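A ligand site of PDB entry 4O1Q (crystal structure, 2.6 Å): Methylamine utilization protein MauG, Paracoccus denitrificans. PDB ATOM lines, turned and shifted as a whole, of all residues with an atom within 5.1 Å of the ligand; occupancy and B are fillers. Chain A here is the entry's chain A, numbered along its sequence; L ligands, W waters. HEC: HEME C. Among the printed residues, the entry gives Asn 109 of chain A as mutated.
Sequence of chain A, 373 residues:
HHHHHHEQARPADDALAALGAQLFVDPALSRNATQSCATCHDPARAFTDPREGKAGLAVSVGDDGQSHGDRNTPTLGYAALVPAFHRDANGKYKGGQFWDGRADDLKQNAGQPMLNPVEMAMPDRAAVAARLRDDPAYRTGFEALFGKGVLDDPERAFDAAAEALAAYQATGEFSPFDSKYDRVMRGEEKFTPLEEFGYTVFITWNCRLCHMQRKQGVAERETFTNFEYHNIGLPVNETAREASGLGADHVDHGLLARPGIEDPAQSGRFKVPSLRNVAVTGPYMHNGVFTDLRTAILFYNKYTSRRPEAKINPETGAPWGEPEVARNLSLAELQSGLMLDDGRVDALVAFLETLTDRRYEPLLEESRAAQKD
CAB of the ligand is covalently linked to SG of Cys 37 (1.8 Å). A carbon (CAC) of the ligand is covalently linked to the side-chain sulfur of Cys 40, 1.8 Å away. NE2 of His 41 is bound to FE of the ligand (2.3 Å). The guanidinium group of Arg 102 lies within salt-bridge range of an oxygen (O2D) of the ligand (2.8 Å). N of Phe 98 lies within hydrogen-bond range of O1A of the ligand (2.8 Å). N of Trp 99 sits at hydrogen-bond distance from O1D of the ligand, at 2.8 Å. O2D of the ligand is in salt-bridge range of NH1 of Arg 71, 3.1 Å away. The side-chain amino group (NZ) of Lys 271 is in salt-bridge range of an oxygen (O2A) of the ligand, 3.4 Å away.
O of Phe 24 lies within hydrogen-bond range of N of Cys 37, at 3.0 Å. O of Pro 74 lies close to ND1 of His 41. O of Asn 72 is in hydrogen-bond range of NE1 of Trp 99 (2.8 Å). The side-chain hydroxyl of Ser 60 sits at hydrogen-bond distance from the side-chain hydroxyl of Thr 73 (2.6 Å). The guanidinium group of Arg 71 lies within salt-bridge range of the side-chain carboxylate of Asp 100, at 2.8 Å. The backbone carbonyl oxygen of Pro 113 is in hydrogen-bond range of the backbone NH of Met 120 (3.1 Å). The side-chain amide nitrogen (NE2) of Gln 35 lies close to the backbone carbonyl oxygen (O) of Glu 119 (3.3 Å). The backbone carbonyl oxygen of Val 61 sits close to the side-chain amide oxygen of Gln 35.
Gln 35 touches the ligand. O of Ser 36 touches CMC of the ligand, at 3.5 Å. Ser 60 touches the ligand. Val 61 touches the ligand. Asn 72 touches the ligand (O to CAD, 3.4 Å). Thr 73 touches the ligand. Pro 74 touches the ligand (CD to C3D, 3.3 Å). Leu 76 touches the ligand (CD2 to C4A, 3.4 Å). Gln 97 touches the ligand. Leu 106 touches the ligand (CD2 to CMA, 3.5 Å). Asn 109 touches the ligand (OD1 to C2A, 3.0 Å). O of Ala 110 touches CBB of the ligand, at 3.6 Å. Pro 113 touches the ligand. Met 114 touches the ligand (CE to CBB, 3.8 Å). OE1 of Glu 119 touches CHD of the ligand, 3.4 Å away. CG of Met 120 touches CMC of the ligand, at 3.3 Å. CD1 of Leu 165 touches CBB of the ligand, 3.5 Å away. OE1 of Gln 169 touches CMB of the ligand (3.2 Å). Hydrophobic or aromatic side chains within 4 Å of the ligand: His 41, Pro 74, Leu 76, Phe 98, Trp 99, Leu 106, Pro 113, Met 114, Met 120 and Leu 165.
Water W1 bridges O of Val 118 (2.7 Å) and O of Ser 60 (2.8 Å).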
ATOM      1  N   PHE A  24     -24.939  -8.597  12.552  1.00  0.00           N
ATOM      2  CA  PHE A  24     -23.561  -8.470  12.985  1.00  0.00           C
ATOM      3  C   PHE A  24     -22.988  -9.814  13.420  1.00  0.00           C
ATOM      4  O   PHE A  24     -21.848 -10.137  13.120  1.00  0.00           O
ATOM      5  CB  PHE A  24     -23.465  -7.463  14.143  1.00  0.00           C
ATOM      6  CG  PHE A  24     -22.060  -7.087  14.499  1.00  0.00           C
ATOM      7  CD1 PHE A  24     -21.369  -6.171  13.739  1.00  0.00           C
ATOM      8  CD2 PHE A  24     -21.437  -7.634  15.604  1.00  0.00           C
ATOM      9  CE1 PHE A  24     -20.074  -5.810  14.062  1.00  0.00           C
ATOM     10  CE2 PHE A  24     -20.143  -7.273  15.942  1.00  0.00           C
ATOM     11  CZ  PHE A  24     -19.459  -6.364  15.167  1.00  0.00           C
ATOM     12  N   GLN A  35     -18.257 -17.393   9.170  1.00  0.00           N
ATOM     13  CA  GLN A  35     -17.892 -16.169   9.892  1.00  0.00           C
ATOM     14  C   GLN A  35     -18.884 -15.001   9.713  1.00  0.00           C
ATOM     15  O   GLN A  35     -19.470 -14.817   8.654  1.00  0.00           O
ATOM     16  CB  GLN A  35     -16.459 -15.736   9.519  1.00  0.00           C
ATOM     17  CG  GLN A  35     -16.296 -14.908   8.248  1.00  0.00           C
ATOM     18  CD  GLN A  35     -14.850 -14.486   8.016  1.00  0.00           C
ATOM     19  OE1 GLN A  35     -13.946 -14.886   8.754  1.00  0.00           O
ATOM     20  NE2 GLN A  35     -14.622 -13.693   6.976  1.00  0.00           N
ATOM     21  N   SER A  36     -19.031 -14.234  10.791  1.00  0.00           N
ATOM     22  CA  SER A  36     -19.879 -13.054  10.849  1.00  0.00           C
ATOM     23  C   SER A  36     -18.985 -11.837  11.083  1.00  0.00           C
ATOM     24  O   SER A  36     -17.764 -11.989  11.143  1.00  0.00           O
ATOM     25  CB  SER A  36     -20.859 -13.209  12.019  1.00  0.00           C
ATOM     26  OG  SER A  36     -20.164 -13.287  13.252  1.00  0.00           O
ATOM     27  N   CYS A  37     -19.576 -10.653  11.220  1.00  0.00           N
ATOM     28  CA  CYS A  37     -18.797  -9.470  11.626  1.00  0.00           C
ATOM     29  C   CYS A  37     -18.117  -9.749  12.965  1.00  0.00           C
ATOM     30  O   CYS A  37     -16.947  -9.404  13.164  1.00  0.00           O
ATOM     31  CB  CYS A  37     -19.675  -8.226  11.799  1.00  0.00           C
ATOM     32  SG  CYS A  37     -20.713  -7.796  10.442  1.00  0.00           S
ATOM     33  N   CYS A  40     -14.403 -11.412  13.106  1.00  0.00           N
ATOM     34  CA  CYS A  40     -13.227 -10.549  12.970  1.00  0.00           C
ATOM     35  C   CYS A  40     -13.326  -9.337  13.887  1.00  0.00           C
ATOM     36  O   CYS A  40     -12.300  -8.774  14.268  1.00  0.00           O
ATOM     37  CB  CYS A  40     -13.066 -10.075  11.519  1.00  0.00           C
ATOM     38  SG  CYS A  40     -12.501 -11.339  10.399  1.00  0.00           S
ATOM     39  N   HIS A  41     -14.554  -8.933  14.225  1.00  0.00           N
ATOM     40  CA  HIS A  41     -14.776  -7.808  15.137  1.00  0.00           C
ATOM     41  C   HIS A  41     -15.481  -8.288  16.396  1.00  0.00           C
ATOM     42  O   HIS A  41     -16.656  -7.987  16.633  1.00  0.00           O
ATOM     43  CB  HIS A  41     -15.595  -6.704  14.466  1.00  0.00           C
ATOM     44  CG  HIS A  41     -14.898  -6.051  13.314  1.00  0.00           C
ATOM     45  ND1 HIS A  41     -13.858  -5.169  13.492  1.00  0.00           N
ATOM     46  CD2 HIS A  41     -15.095  -6.145  11.981  1.00  0.00           C
ATOM     47  CE1 HIS A  41     -13.450  -4.735  12.311  1.00  0.00           C
ATOM     48  NE2 HIS A  41     -14.187  -5.313  11.377  1.00  0.00           N
ATOM     49  N   ARG A  51      -8.542 -14.275  16.650  1.00  0.00           N
ATOM     50  CA  ARG A  51      -8.041 -15.447  15.922  1.00  0.00           C
ATOM     51  C   ARG A  51      -6.629 -15.259  15.378  1.00  0.00           C
ATOM     52  O   ARG A  51      -6.222 -14.130  15.100  1.00  0.00           O
ATOM     53  CB  ARG A  51      -8.975 -15.786  14.762  1.00  0.00           C
ATOM     54  CG  ARG A  51     -10.440 -16.009  15.144  1.00  0.00           C
ATOM     55  CD  ARG A  51     -11.274 -16.281  13.904  1.00  0.00           C
ATOM     56  NE  ARG A  51     -11.154 -15.195  12.932  1.00  0.00           N
ATOM     57  CZ  ARG A  51     -11.351 -15.317  11.621  1.00  0.00           C
ATOM     58  NH1 ARG A  51     -11.692 -16.475  11.076  1.00  0.00           N
ATOM     59  NH2 ARG A  51     -11.195 -14.251  10.840  1.00  0.00           N
ATOM     60  N   SER A  60      -6.447 -10.968   9.640  1.00  0.00           N
ATOM     61  CA  SER A  60      -7.549 -11.892   9.909  1.00  0.00           C
ATOM     62  C   SER A  60      -7.704 -12.879   8.767  1.00  0.00           C
ATOM     63  O   SER A  60      -7.330 -12.584   7.635  1.00  0.00           O
ATOM     64  CB  SER A  60      -8.856 -11.113  10.082  1.00  0.00           C
ATOM     65  OG  SER A  60      -8.825 -10.270  11.219  1.00  0.00           O
ATOM     66  N   VAL A  61      -8.240 -14.060   9.083  1.00  0.00           N
ATOM     67  CA  VAL A  61      -8.475 -15.106   8.084  1.00  0.00           C
ATOM     68  C   VAL A  61      -9.904 -15.017   7.547  1.00  0.00           C
ATOM     69  O   VAL A  61     -10.851 -14.790   8.302  1.00  0.00           O
ATOM     70  CB  VAL A  61      -8.248 -16.515   8.662  1.00  0.00           C
ATOM     71  CG1 VAL A  61      -8.260 -17.553   7.551  1.00  0.00           C
ATOM     72  CG2 VAL A  61      -6.936 -16.547   9.427  1.00  0.00           C
ATOM     73  N   GLY A  62     -10.044 -15.231   6.241  1.00  0.00           N
ATOM     74  CA  GLY A  62     -11.333 -15.134   5.581  1.00  0.00           C
ATOM     75  C   GLY A  62     -12.250 -16.301   5.864  1.00  0.00           C
ATOM     76  O   GLY A  62     -11.938 -17.165   6.678  1.00  0.00           O
ATOM     77  N   ARG A  71      -4.061  -5.951   5.988  1.00  0.00           N
ATOM     78  CA  ARG A  71      -4.113  -4.962   7.065  1.00  0.00           C
ATOM     79  C   ARG A  71      -4.753  -5.527   8.329  1.00  0.00           C
ATOM     80  O   ARG A  71      -5.504  -6.512   8.284  1.00  0.00           O
ATOM     81  CB  ARG A  71      -4.870  -3.701   6.598  1.00  0.00           C
ATOM     82  CG  ARG A  71      -4.284  -3.033   5.365  1.00  0.00           C
ATOM     83  CD  ARG A  71      -4.675  -1.570   5.293  1.00  0.00           C
ATOM     84  NE  ARG A  71      -4.136  -0.879   4.111  1.00  0.00           N
ATOM     85  CZ  ARG A  71      -4.864  -0.395   3.093  1.00  0.00           C
ATOM     86  NH1 ARG A  71      -6.190  -0.495   3.076  1.00  0.00           N
ATOM     87  NH2 ARG A  71      -4.249   0.217   2.084  1.00  0.00           N
ATOM     88  N   ASN A  72      -4.431  -4.896   9.457  1.00  0.00           N
ATOM     89  CA  ASN A  72      -4.947  -5.299  10.755  1.00  0.00           C
ATOM     90  C   ASN A  72      -6.389  -4.829  10.950  1.00  0.00           C
ATOM     91  O   ASN A  72      -6.757  -3.720  10.550  1.00  0.00           O
ATOM     92  CB  ASN A  72      -4.055  -4.738  11.868  1.00  0.00           C
ATOM     93  CG  ASN A  72      -4.578  -5.073  13.251  1.00  0.00           C
ATOM     94  OD1 ASN A  72      -4.991  -4.187  14.004  1.00  0.00           O
ATOM     95  ND2 ASN A  72      -4.563  -6.362  13.595  1.00  0.00           N
ATOM     96  N   THR A  73      -7.187  -5.676  11.594  1.00  0.00           N
ATOM     97  CA  THR A  73      -8.583  -5.387  11.850  1.00  0.00           C
ATOM     98  C   THR A  73      -8.704  -4.367  12.986  1.00  0.00           C
ATOM     99  O   THR A  73      -8.217  -4.605  14.089  1.00  0.00           O
ATOM    100  CB  THR A  73      -9.359  -6.677  12.200  1.00  0.00           C
ATOM    101  OG1 THR A  73      -9.022  -7.705  11.264  1.00  0.00           O
ATOM    102  CG2 THR A  73     -10.852  -6.450  12.162  1.00  0.00           C
ATOM    103  N   PRO A  74      -9.335  -3.207  12.713  1.00  0.00           N
ATOM    104  CA  PRO A  74      -9.459  -2.157  13.714  1.00  0.00           C
ATOM    105  C   PRO A  74     -10.707  -2.309  14.572  1.00  0.00           C
ATOM    106  O   PRO A  74     -11.676  -2.935  14.147  1.00  0.00           O
ATOM    107  CB  PRO A  74      -9.570  -0.893  12.856  1.00  0.00           C
ATOM    108  CG  PRO A  74     -10.301  -1.350  11.648  1.00  0.00           C
ATOM    109  CD  PRO A  74      -9.884  -2.789  11.414  1.00  0.00           C
ATOM    110  N   THR A  75     -10.687  -1.719  15.758  1.00  0.00           N
ATOM    111  CA  THR A  75     -11.901  -1.587  16.560  1.00  0.00           C
ATOM    112  C   THR A  75     -13.015  -0.946  15.737  1.00  0.00           C
ATOM    113  O   THR A  75     -12.757  -0.139  14.845  1.00  0.00           O
ATOM    114  CB  THR A  75     -11.643  -0.751  17.833  1.00  0.00           C
ATOM    115  OG1 THR A  75     -12.794  -0.802  18.682  1.00  0.00           O
ATOM    116  CG2 THR A  75     -11.322   0.705  17.503  1.00  0.00           C
ATOM    117  N   LEU A  76     -14.251  -1.358  16.013  1.00  0.00           N
ATOM    118  CA  LEU A  76     -15.426  -0.676  15.496  1.00  0.00           C
ATOM    119  C   LEU A  76     -15.873   0.384  16.491  1.00  0.00           C
ATOM    120  O   LEU A  76     -16.566   1.344  16.127  1.00  0.00           O
ATOM    121  CB  LEU A  76     -16.564  -1.645  15.235  1.00  0.00           C
ATOM    122  CG  LEU A  76     -16.268  -2.778  14.250  1.00  0.00           C
ATOM    123  CD1 LEU A  76     -17.555  -3.487  13.846  1.00  0.00           C
ATOM    124  CD2 LEU A  76     -15.526  -2.293  13.011  1.00  0.00           C
ATOM    125  N   ALA A  79     -15.879   4.363  15.863  1.00  0.00           N
ATOM    126  CA  ALA A  79     -15.763   4.650  14.433  1.00  0.00           C
ATOM    127  C   ALA A  79     -16.903   5.546  13.953  1.00  0.00           C
ATOM    128  O   ALA A  79     -16.765   6.274  12.971  1.00  0.00           O
ATOM    129  CB  ALA A  79     -15.730   3.364  13.624  1.00  0.00           C
ATOM    130  N   GLN A  97     -13.393   5.715   6.424  1.00  0.00           N
ATOM    131  CA  GLN A  97     -13.293   4.400   7.062  1.00  0.00           C
ATOM    132  C   GLN A  97     -12.312   3.490   6.316  1.00  0.00           C
ATOM    133  O   GLN A  97     -12.086   3.649   5.116  1.00  0.00           O
ATOM    134  CB  GLN A  97     -14.679   3.748   7.135  1.00  0.00           C
ATOM    135  CG  GLN A  97     -15.712   4.540   7.945  1.00  0.00           C
ATOM    136  CD  GLN A  97     -15.419   4.592   9.438  1.00  0.00           C
ATOM    137  OE1 GLN A  97     -15.775   5.563  10.112  1.00  0.00           O
ATOM    138  NE2 GLN A  97     -14.805   3.544   9.966  1.00  0.00           N
ATOM    139  N   PHE A  98     -11.743   2.538   7.052  1.00  0.00           N
ATOM    140  CA  PHE A  98     -10.601   1.711   6.613  1.00  0.00           C
ATOM    141  C   PHE A  98      -9.318   2.508   6.827  1.00  0.00           C
ATOM    142  O   PHE A  98      -9.305   3.741   6.666  1.00  0.00           O
ATOM    143  CB  PHE A  98     -10.668   1.240   5.147  1.00  0.00           C
ATOM    144  CG  PHE A  98     -11.790   0.267   4.857  1.00  0.00           C
ATOM    145  CD1 PHE A  98     -11.858  -0.955   5.501  1.00  0.00           C
ATOM    146  CD2 PHE A  98     -12.742   0.552   3.879  1.00  0.00           C
ATOM    147  CE1 PHE A  98     -12.870  -1.856   5.216  1.00  0.00           C
ATOM    148  CE2 PHE A  98     -13.753  -0.348   3.594  1.00  0.00           C
ATOM    149  CZ  PHE A  98     -13.819  -1.558   4.259  1.00  0.00           C
ATOM    150  N   TRP A  99      -8.227   1.811   7.177  1.00  0.00           N
ATOM    151  CA  TRP A  99      -6.923   2.454   7.403  1.00  0.00           C
ATOM    152  C   TRP A  99      -6.511   3.429   6.310  1.00  0.00           C
ATOM    153  O   TRP A  99      -5.738   4.350   6.566  1.00  0.00           O
ATOM    154  CB  TRP A  99      -5.827   1.392   7.544  1.00  0.00           C
ATOM    155  CG  TRP A  99      -5.907   0.623   8.814  1.00  0.00           C
ATOM    156  CD1 TRP A  99      -6.430  -0.620   8.973  1.00  0.00           C
ATOM    157  CD2 TRP A  99      -5.447   1.049  10.093  1.00  0.00           C
ATOM    158  NE1 TRP A  99      -6.317  -1.009  10.276  1.00  0.00           N
ATOM    159  CE2 TRP A  99      -5.721  -0.005  10.997  1.00  0.00           C
ATOM    160  CE3 TRP A  99      -4.826   2.198  10.573  1.00  0.00           C
ATOM    161  CZ2 TRP A  99      -5.393   0.065  12.347  1.00  0.00           C
ATOM    162  CZ3 TRP A  99      -4.498   2.268  11.924  1.00  0.00           C
ATOM    163  CH2 TRP A  99      -4.785   1.213  12.793  1.00  0.00           C
ATOM    164  N   ASP A 100      -7.017   3.229   5.091  1.00  0.00           N
ATOM    165  CA  ASP A 100      -6.690   4.089   3.957  1.00  0.00           C
ATOM    166  C   ASP A 100      -7.849   5.022   3.562  1.00  0.00           C
ATOM    167  O   ASP A 100      -7.803   5.686   2.526  1.00  0.00           O
ATOM    168  CB  ASP A 100      -6.271   3.231   2.759  1.00  0.00           C
ATOM    169  CG  ASP A 100      -7.367   2.286   2.299  1.00  0.00           C
ATOM    170  OD1 ASP A 100      -8.471   2.296   2.886  1.00  0.00           O
ATOM    171  OD2 ASP A 100      -7.123   1.520   1.339  1.00  0.00           O
ATOM    172  N   ARG A 102     -10.682   4.332   2.377  1.00  0.00           N
ATOM    173  CA  ARG A 102     -11.300   4.001   1.081  1.00  0.00           C
ATOM    174  C   ARG A 102     -12.828   3.884   1.154  1.00  0.00           C
ATOM    175  O   ARG A 102     -13.479   3.756   0.123  1.00  0.00           O
ATOM    176  CB  ARG A 102     -10.695   2.719   0.483  1.00  0.00           C
ATOM    177  CG  ARG A 102     -11.150   1.429   1.122  1.00  0.00           C
ATOM    178  CD  ARG A 102     -10.581   0.213   0.398  1.00  0.00           C
ATOM    179  NE  ARG A 102     -10.830  -1.033   1.110  1.00  0.00           N
ATOM    180  CZ  ARG A 102     -10.193  -1.403   2.223  1.00  0.00           C
ATOM    181  NH1 ARG A 102     -10.486  -2.561   2.802  1.00  0.00           N
ATOM    182  NH2 ARG A 102      -9.263  -0.615   2.771  1.00  0.00           N
ATOM    183  N   LEU A 106     -19.388   4.538   7.557  1.00  0.00           N
ATOM    184  CA  LEU A 106     -19.784   3.211   8.052  1.00  0.00           C
ATOM    185  C   LEU A 106     -20.707   2.451   7.101  1.00  0.00           C
ATOM    186  O   LEU A 106     -20.578   1.235   6.940  1.00  0.00           O
ATOM    187  CB  LEU A 106     -20.469   3.344   9.415  1.00  0.00           C
ATOM    188  CG  LEU A 106     -19.563   3.509  10.624  1.00  0.00           C
ATOM    189  CD1 LEU A 106     -20.332   4.111  11.779  1.00  0.00           C
ATOM    190  CD2 LEU A 106     -18.955   2.171  11.023  1.00  0.00           C
ATOM    191  N   ASN A 109     -18.808   1.228   4.094  1.00  0.00           N
ATOM    192  CA  ASN A 109     -17.833   0.275   4.593  1.00  0.00           C
ATOM    193  C   ASN A 109     -18.411  -1.127   4.803  1.00  0.00           C
ATOM    194  O   ASN A 109     -17.798  -2.119   4.419  1.00  0.00           O
ATOM    195  CB  ASN A 109     -17.228   0.796   5.897  1.00  0.00           C
ATOM    196  CG  ASN A 109     -16.446  -0.268   6.641  1.00  0.00           C
ATOM    197  OD1 ASN A 109     -15.216  -0.255   6.645  1.00  0.00           O
ATOM    198  ND2 ASN A 109     -17.155  -1.196   7.274  1.00  0.00           N
ATOM    199  N   ALA A 110     -19.607  -1.193   5.398  1.00  0.00           N
ATOM    200  CA  ALA A 110     -20.210  -2.461   5.857  1.00  0.00           C
ATOM    201  C   ALA A 110     -20.333  -3.526   4.777  1.00  0.00           C
ATOM    202  O   ALA A 110     -20.221  -4.714   5.069  1.00  0.00           O
ATOM    203  CB  ALA A 110     -21.580  -2.207   6.473  1.00  0.00           C
ATOM    204  N   PRO A 113     -16.672  -6.146   3.392  1.00  0.00           N
ATOM    205  CA  PRO A 113     -16.295  -7.453   3.938  1.00  0.00           C
ATOM    206  C   PRO A 113     -17.140  -8.625   3.399  1.00  0.00           C
ATOM    207  O   PRO A 113     -16.589  -9.667   3.066  1.00  0.00           O
ATOM    208  CB  PRO A 113     -16.532  -7.285   5.438  1.00  0.00           C
ATOM    209  CG  PRO A 113     -16.345  -5.835   5.677  1.00  0.00           C
ATOM    210  CD  PRO A 113     -16.853  -5.150   4.450  1.00  0.00           C
ATOM    211  N   MET A 114     -18.451  -8.420   3.314  1.00  0.00           N
ATOM    212  CA  MET A 114     -19.375  -9.435   2.792  1.00  0.00           C
ATOM    213  C   MET A 114     -18.960  -9.953   1.420  1.00  0.00           C
ATOM    214  O   MET A 114     -19.057 -11.134   1.145  1.00  0.00           O
ATOM    215  CB  MET A 114     -20.805  -8.896   2.698  1.00  0.00           C
ATOM    216  CG  MET A 114     -21.437  -8.540   4.032  1.00  0.00           C
ATOM    217  SD  MET A 114     -23.139  -7.990   3.825  1.00  0.00           S
ATOM    218  CE  MET A 114     -23.430  -7.189   5.394  1.00  0.00           C
ATOM    219  N   VAL A 118     -11.256 -12.606   0.087  1.00  0.00           N
ATOM    220  CA  VAL A 118     -10.328 -12.879   1.179  1.00  0.00           C
ATOM    221  C   VAL A 118     -10.926 -12.560   2.562  1.00  0.00           C
ATOM    222  O   VAL A 118     -10.212 -12.604   3.576  1.00  0.00           O
ATOM    223  CB  VAL A 118      -8.949 -12.163   0.987  1.00  0.00           C
ATOM    224  CG1 VAL A 118      -8.360 -12.530  -0.367  1.00  0.00           C
ATOM    225  CG2 VAL A 118      -9.052 -10.652   1.135  1.00  0.00           C
ATOM    226  N   GLU A 119     -12.213 -12.231   2.611  1.00  0.00           N
ATOM    227  CA  GLU A 119     -12.944 -12.108   3.869  1.00  0.00           C
ATOM    228  C   GLU A 119     -14.207 -12.998   3.830  1.00  0.00           C
ATOM    229  O   GLU A 119     -14.080 -14.210   3.747  1.00  0.00           O
ATOM    230  CB  GLU A 119     -13.222 -10.641   4.212  1.00  0.00           C
ATOM    231  CG  GLU A 119     -11.947  -9.808   4.285  1.00  0.00           C
ATOM    232  CD  GLU A 119     -12.191  -8.334   4.564  1.00  0.00           C
ATOM    233  OE1 GLU A 119     -11.759  -7.852   5.631  1.00  0.00           O
ATOM    234  OE2 GLU A 119     -12.789  -7.648   3.707  1.00  0.00           O
ATOM    235  N   MET A 120     -15.409 -12.407   3.872  1.00  0.00           N
ATOM    236  CA  MET A 120     -16.647 -13.203   3.990  1.00  0.00           C
ATOM    237  C   MET A 120     -16.977 -13.990   2.719  1.00  0.00           C
ATOM    238  O   MET A 120     -17.694 -14.995   2.779  1.00  0.00           O
ATOM    239  CB  MET A 120     -17.821 -12.326   4.401  1.00  0.00           C
ATOM    240  CG  MET A 120     -17.583 -11.587   5.716  1.00  0.00           C
ATOM    241  SD  MET A 120     -18.995 -10.699   6.395  1.00  0.00           S
ATOM    242  CE  MET A 120     -19.811 -11.977   7.361  1.00  0.00           C
ATOM    243  N   LEU A 165     -26.382  -2.376   9.869  1.00  0.00           N
ATOM    244  CA  LEU A 165     -25.063  -2.580  10.470  1.00  0.00           C
ATOM    245  C   LEU A 165     -24.397  -1.261  10.859  1.00  0.00           C
ATOM    246  O   LEU A 165     -23.830  -1.144  11.942  1.00  0.00           O
ATOM    247  CB  LEU A 165     -24.168  -3.371   9.530  1.00  0.00           C
ATOM    248  CG  LEU A 165     -24.513  -4.854   9.421  1.00  0.00           C
ATOM    249  CD1 LEU A 165     -23.897  -5.470   8.177  1.00  0.00           C
ATOM    250  CD2 LEU A 165     -24.068  -5.618  10.663  1.00  0.00           C
ATOM    251  N   GLN A 169     -23.698   0.136  14.728  1.00  0.00           N
ATOM    252  CA  GLN A 169     -22.407   0.665  15.166  1.00  0.00           C
ATOM    253  C   GLN A 169     -22.458   2.126  15.645  1.00  0.00           C
ATOM    254  O   GLN A 169     -21.493   2.627  16.226  1.00  0.00           O
ATOM    255  CB  GLN A 169     -21.378   0.534  14.050  1.00  0.00           C
ATOM    256  CG  GLN A 169     -21.057  -0.893  13.664  1.00  0.00           C
ATOM    257  CD  GLN A 169     -20.261  -0.983  12.384  1.00  0.00           C
ATOM    258  OE1 GLN A 169     -20.818  -1.197  11.307  1.00  0.00           O
ATOM    259  NE2 GLN A 169     -18.951  -0.804  12.486  1.00  0.00           N
ATOM    260  N   LYS A 271      -5.071   6.644   7.939  1.00  0.00           N
ATOM    261  CA  LYS A 271      -5.940   7.363   8.864  1.00  0.00           C
ATOM    262  C   LYS A 271      -5.366   7.302  10.271  1.00  0.00           C
ATOM    263  O   LYS A 271      -4.844   6.277  10.696  1.00  0.00           O
ATOM    264  CB  LYS A 271      -7.347   6.762   8.874  1.00  0.00           C
ATOM    265  CG  LYS A 271      -8.352   7.539   9.726  1.00  0.00           C
ATOM    266  CD  LYS A 271      -9.792   7.100   9.462  1.00  0.00           C
ATOM    267  CE  LYS A 271     -10.048   5.635   9.840  1.00  0.00           C
ATOM    268  NZ  LYS A 271      -9.705   5.322  11.251  1.00  0.00           N
HETATM  269 FE   HEC L   1     -14.395  -5.252   9.098  1.00  0.00          FE
HETATM  270  CHA HEC L   1     -12.186  -2.657   8.616  1.00  0.00           C
HETATM  271  CHB HEC L   1     -16.918  -3.045   9.957  1.00  0.00           C
HETATM  272  CHC HEC L   1     -16.727  -7.759   8.693  1.00  0.00           C
HETATM  273  CHD HEC L   1     -11.830  -7.577   8.974  1.00  0.00           C
HETATM  274  NA  HEC L   1     -14.525  -3.168   9.251  1.00  0.00           N
HETATM  275  C1A HEC L   1     -13.550  -2.267   9.028  1.00  0.00           C
HETATM  276  C2A HEC L   1     -13.962  -0.862   9.275  1.00  0.00           C
HETATM  277  C3A HEC L   1     -15.365  -0.989   9.685  1.00  0.00           C
HETATM  278  C4A HEC L   1     -15.586  -2.457   9.659  1.00  0.00           C
HETATM  279  CMA HEC L   1     -16.342   0.100  10.057  1.00  0.00           C
HETATM  280  CAA HEC L   1     -13.164   0.422   9.152  1.00  0.00           C
HETATM  281  CBA HEC L   1     -12.867   0.924  10.577  1.00  0.00           C
HETATM  282  CGA HEC L   1     -11.707   1.910  10.675  1.00  0.00           C
HETATM  283  O1A HEC L   1     -10.966   2.107   9.681  1.00  0.00           O
HETATM  284  O2A HEC L   1     -11.531   2.492  11.771  1.00  0.00           O
HETATM  285  NB  HEC L   1     -16.475  -5.373   9.278  1.00  0.00           N
HETATM  286  C1B HEC L   1     -17.344  -4.415   9.646  1.00  0.00           C
HETATM  287  C2B HEC L   1     -18.776  -4.856   9.665  1.00  0.00           C
HETATM  288  C3B HEC L   1     -18.702  -6.281   9.285  1.00  0.00           C
HETATM  289  C4B HEC L   1     -17.249  -6.441   9.056  1.00  0.00           C
HETATM  290  CMB HEC L   1     -19.993  -4.038  10.006  1.00  0.00           C
HETATM  291  CAB HEC L   1     -19.743  -7.355   9.049  1.00  0.00           C
HETATM  292  CBB HEC L   1     -20.644  -6.863   7.929  1.00  0.00           C
HETATM  293  NC  HEC L   1     -14.294  -7.321   8.861  1.00  0.00           N
HETATM  294  C1C HEC L   1     -15.330  -8.162   8.726  1.00  0.00           C
HETATM  295  C2C HEC L   1     -14.975  -9.576   8.628  1.00  0.00           C
HETATM  296  C3C HEC L   1     -13.508  -9.568   8.690  1.00  0.00           C
HETATM  297  C4C HEC L   1     -13.202  -8.114   8.891  1.00  0.00           C
HETATM  298  CMC HEC L   1     -15.898 -10.745   8.466  1.00  0.00           C
HETATM  299  CAC HEC L   1     -12.663 -10.830   8.702  1.00  0.00           C
HETATM  300  CBC HEC L   1     -11.633 -11.270   7.654  1.00  0.00           C
HETATM  301  ND  HEC L   1     -12.341  -5.133   8.821  1.00  0.00           N
HETATM  302  C1D HEC L   1     -11.444  -6.143   8.812  1.00  0.00           C
HETATM  303  C2D HEC L   1     -10.045  -5.715   8.575  1.00  0.00           C
HETATM  304  C3D HEC L   1     -10.179  -4.264   8.483  1.00  0.00           C
HETATM  305  C4D HEC L   1     -11.624  -4.027   8.620  1.00  0.00           C
HETATM  306  CMD HEC L   1      -8.768  -6.505   8.459  1.00  0.00           C
HETATM  307  CAD HEC L   1      -9.106  -3.250   8.173  1.00  0.00           C
HETATM  308  CBD HEC L   1      -9.198  -3.211   6.648  1.00  0.00           C
HETATM  309  CGD HEC L   1      -8.627  -1.987   5.991  1.00  0.00           C
HETATM  310  O1D HEC L   1      -8.625  -0.904   6.608  1.00  0.00           O
HETATM  311  O2D HEC L   1      -8.192  -2.126   4.819  1.00  0.00           O
HETATM  312  O   HOH W   1      -8.874 -11.387   5.617  1.00  0.00           O
HETATM  313  O   HOH W   2     -15.854  -3.284   6.809  1.00  0.00           O
HETATM  314  O   HOH W   3     -12.727  -5.346   6.028  1.00  0.00           O
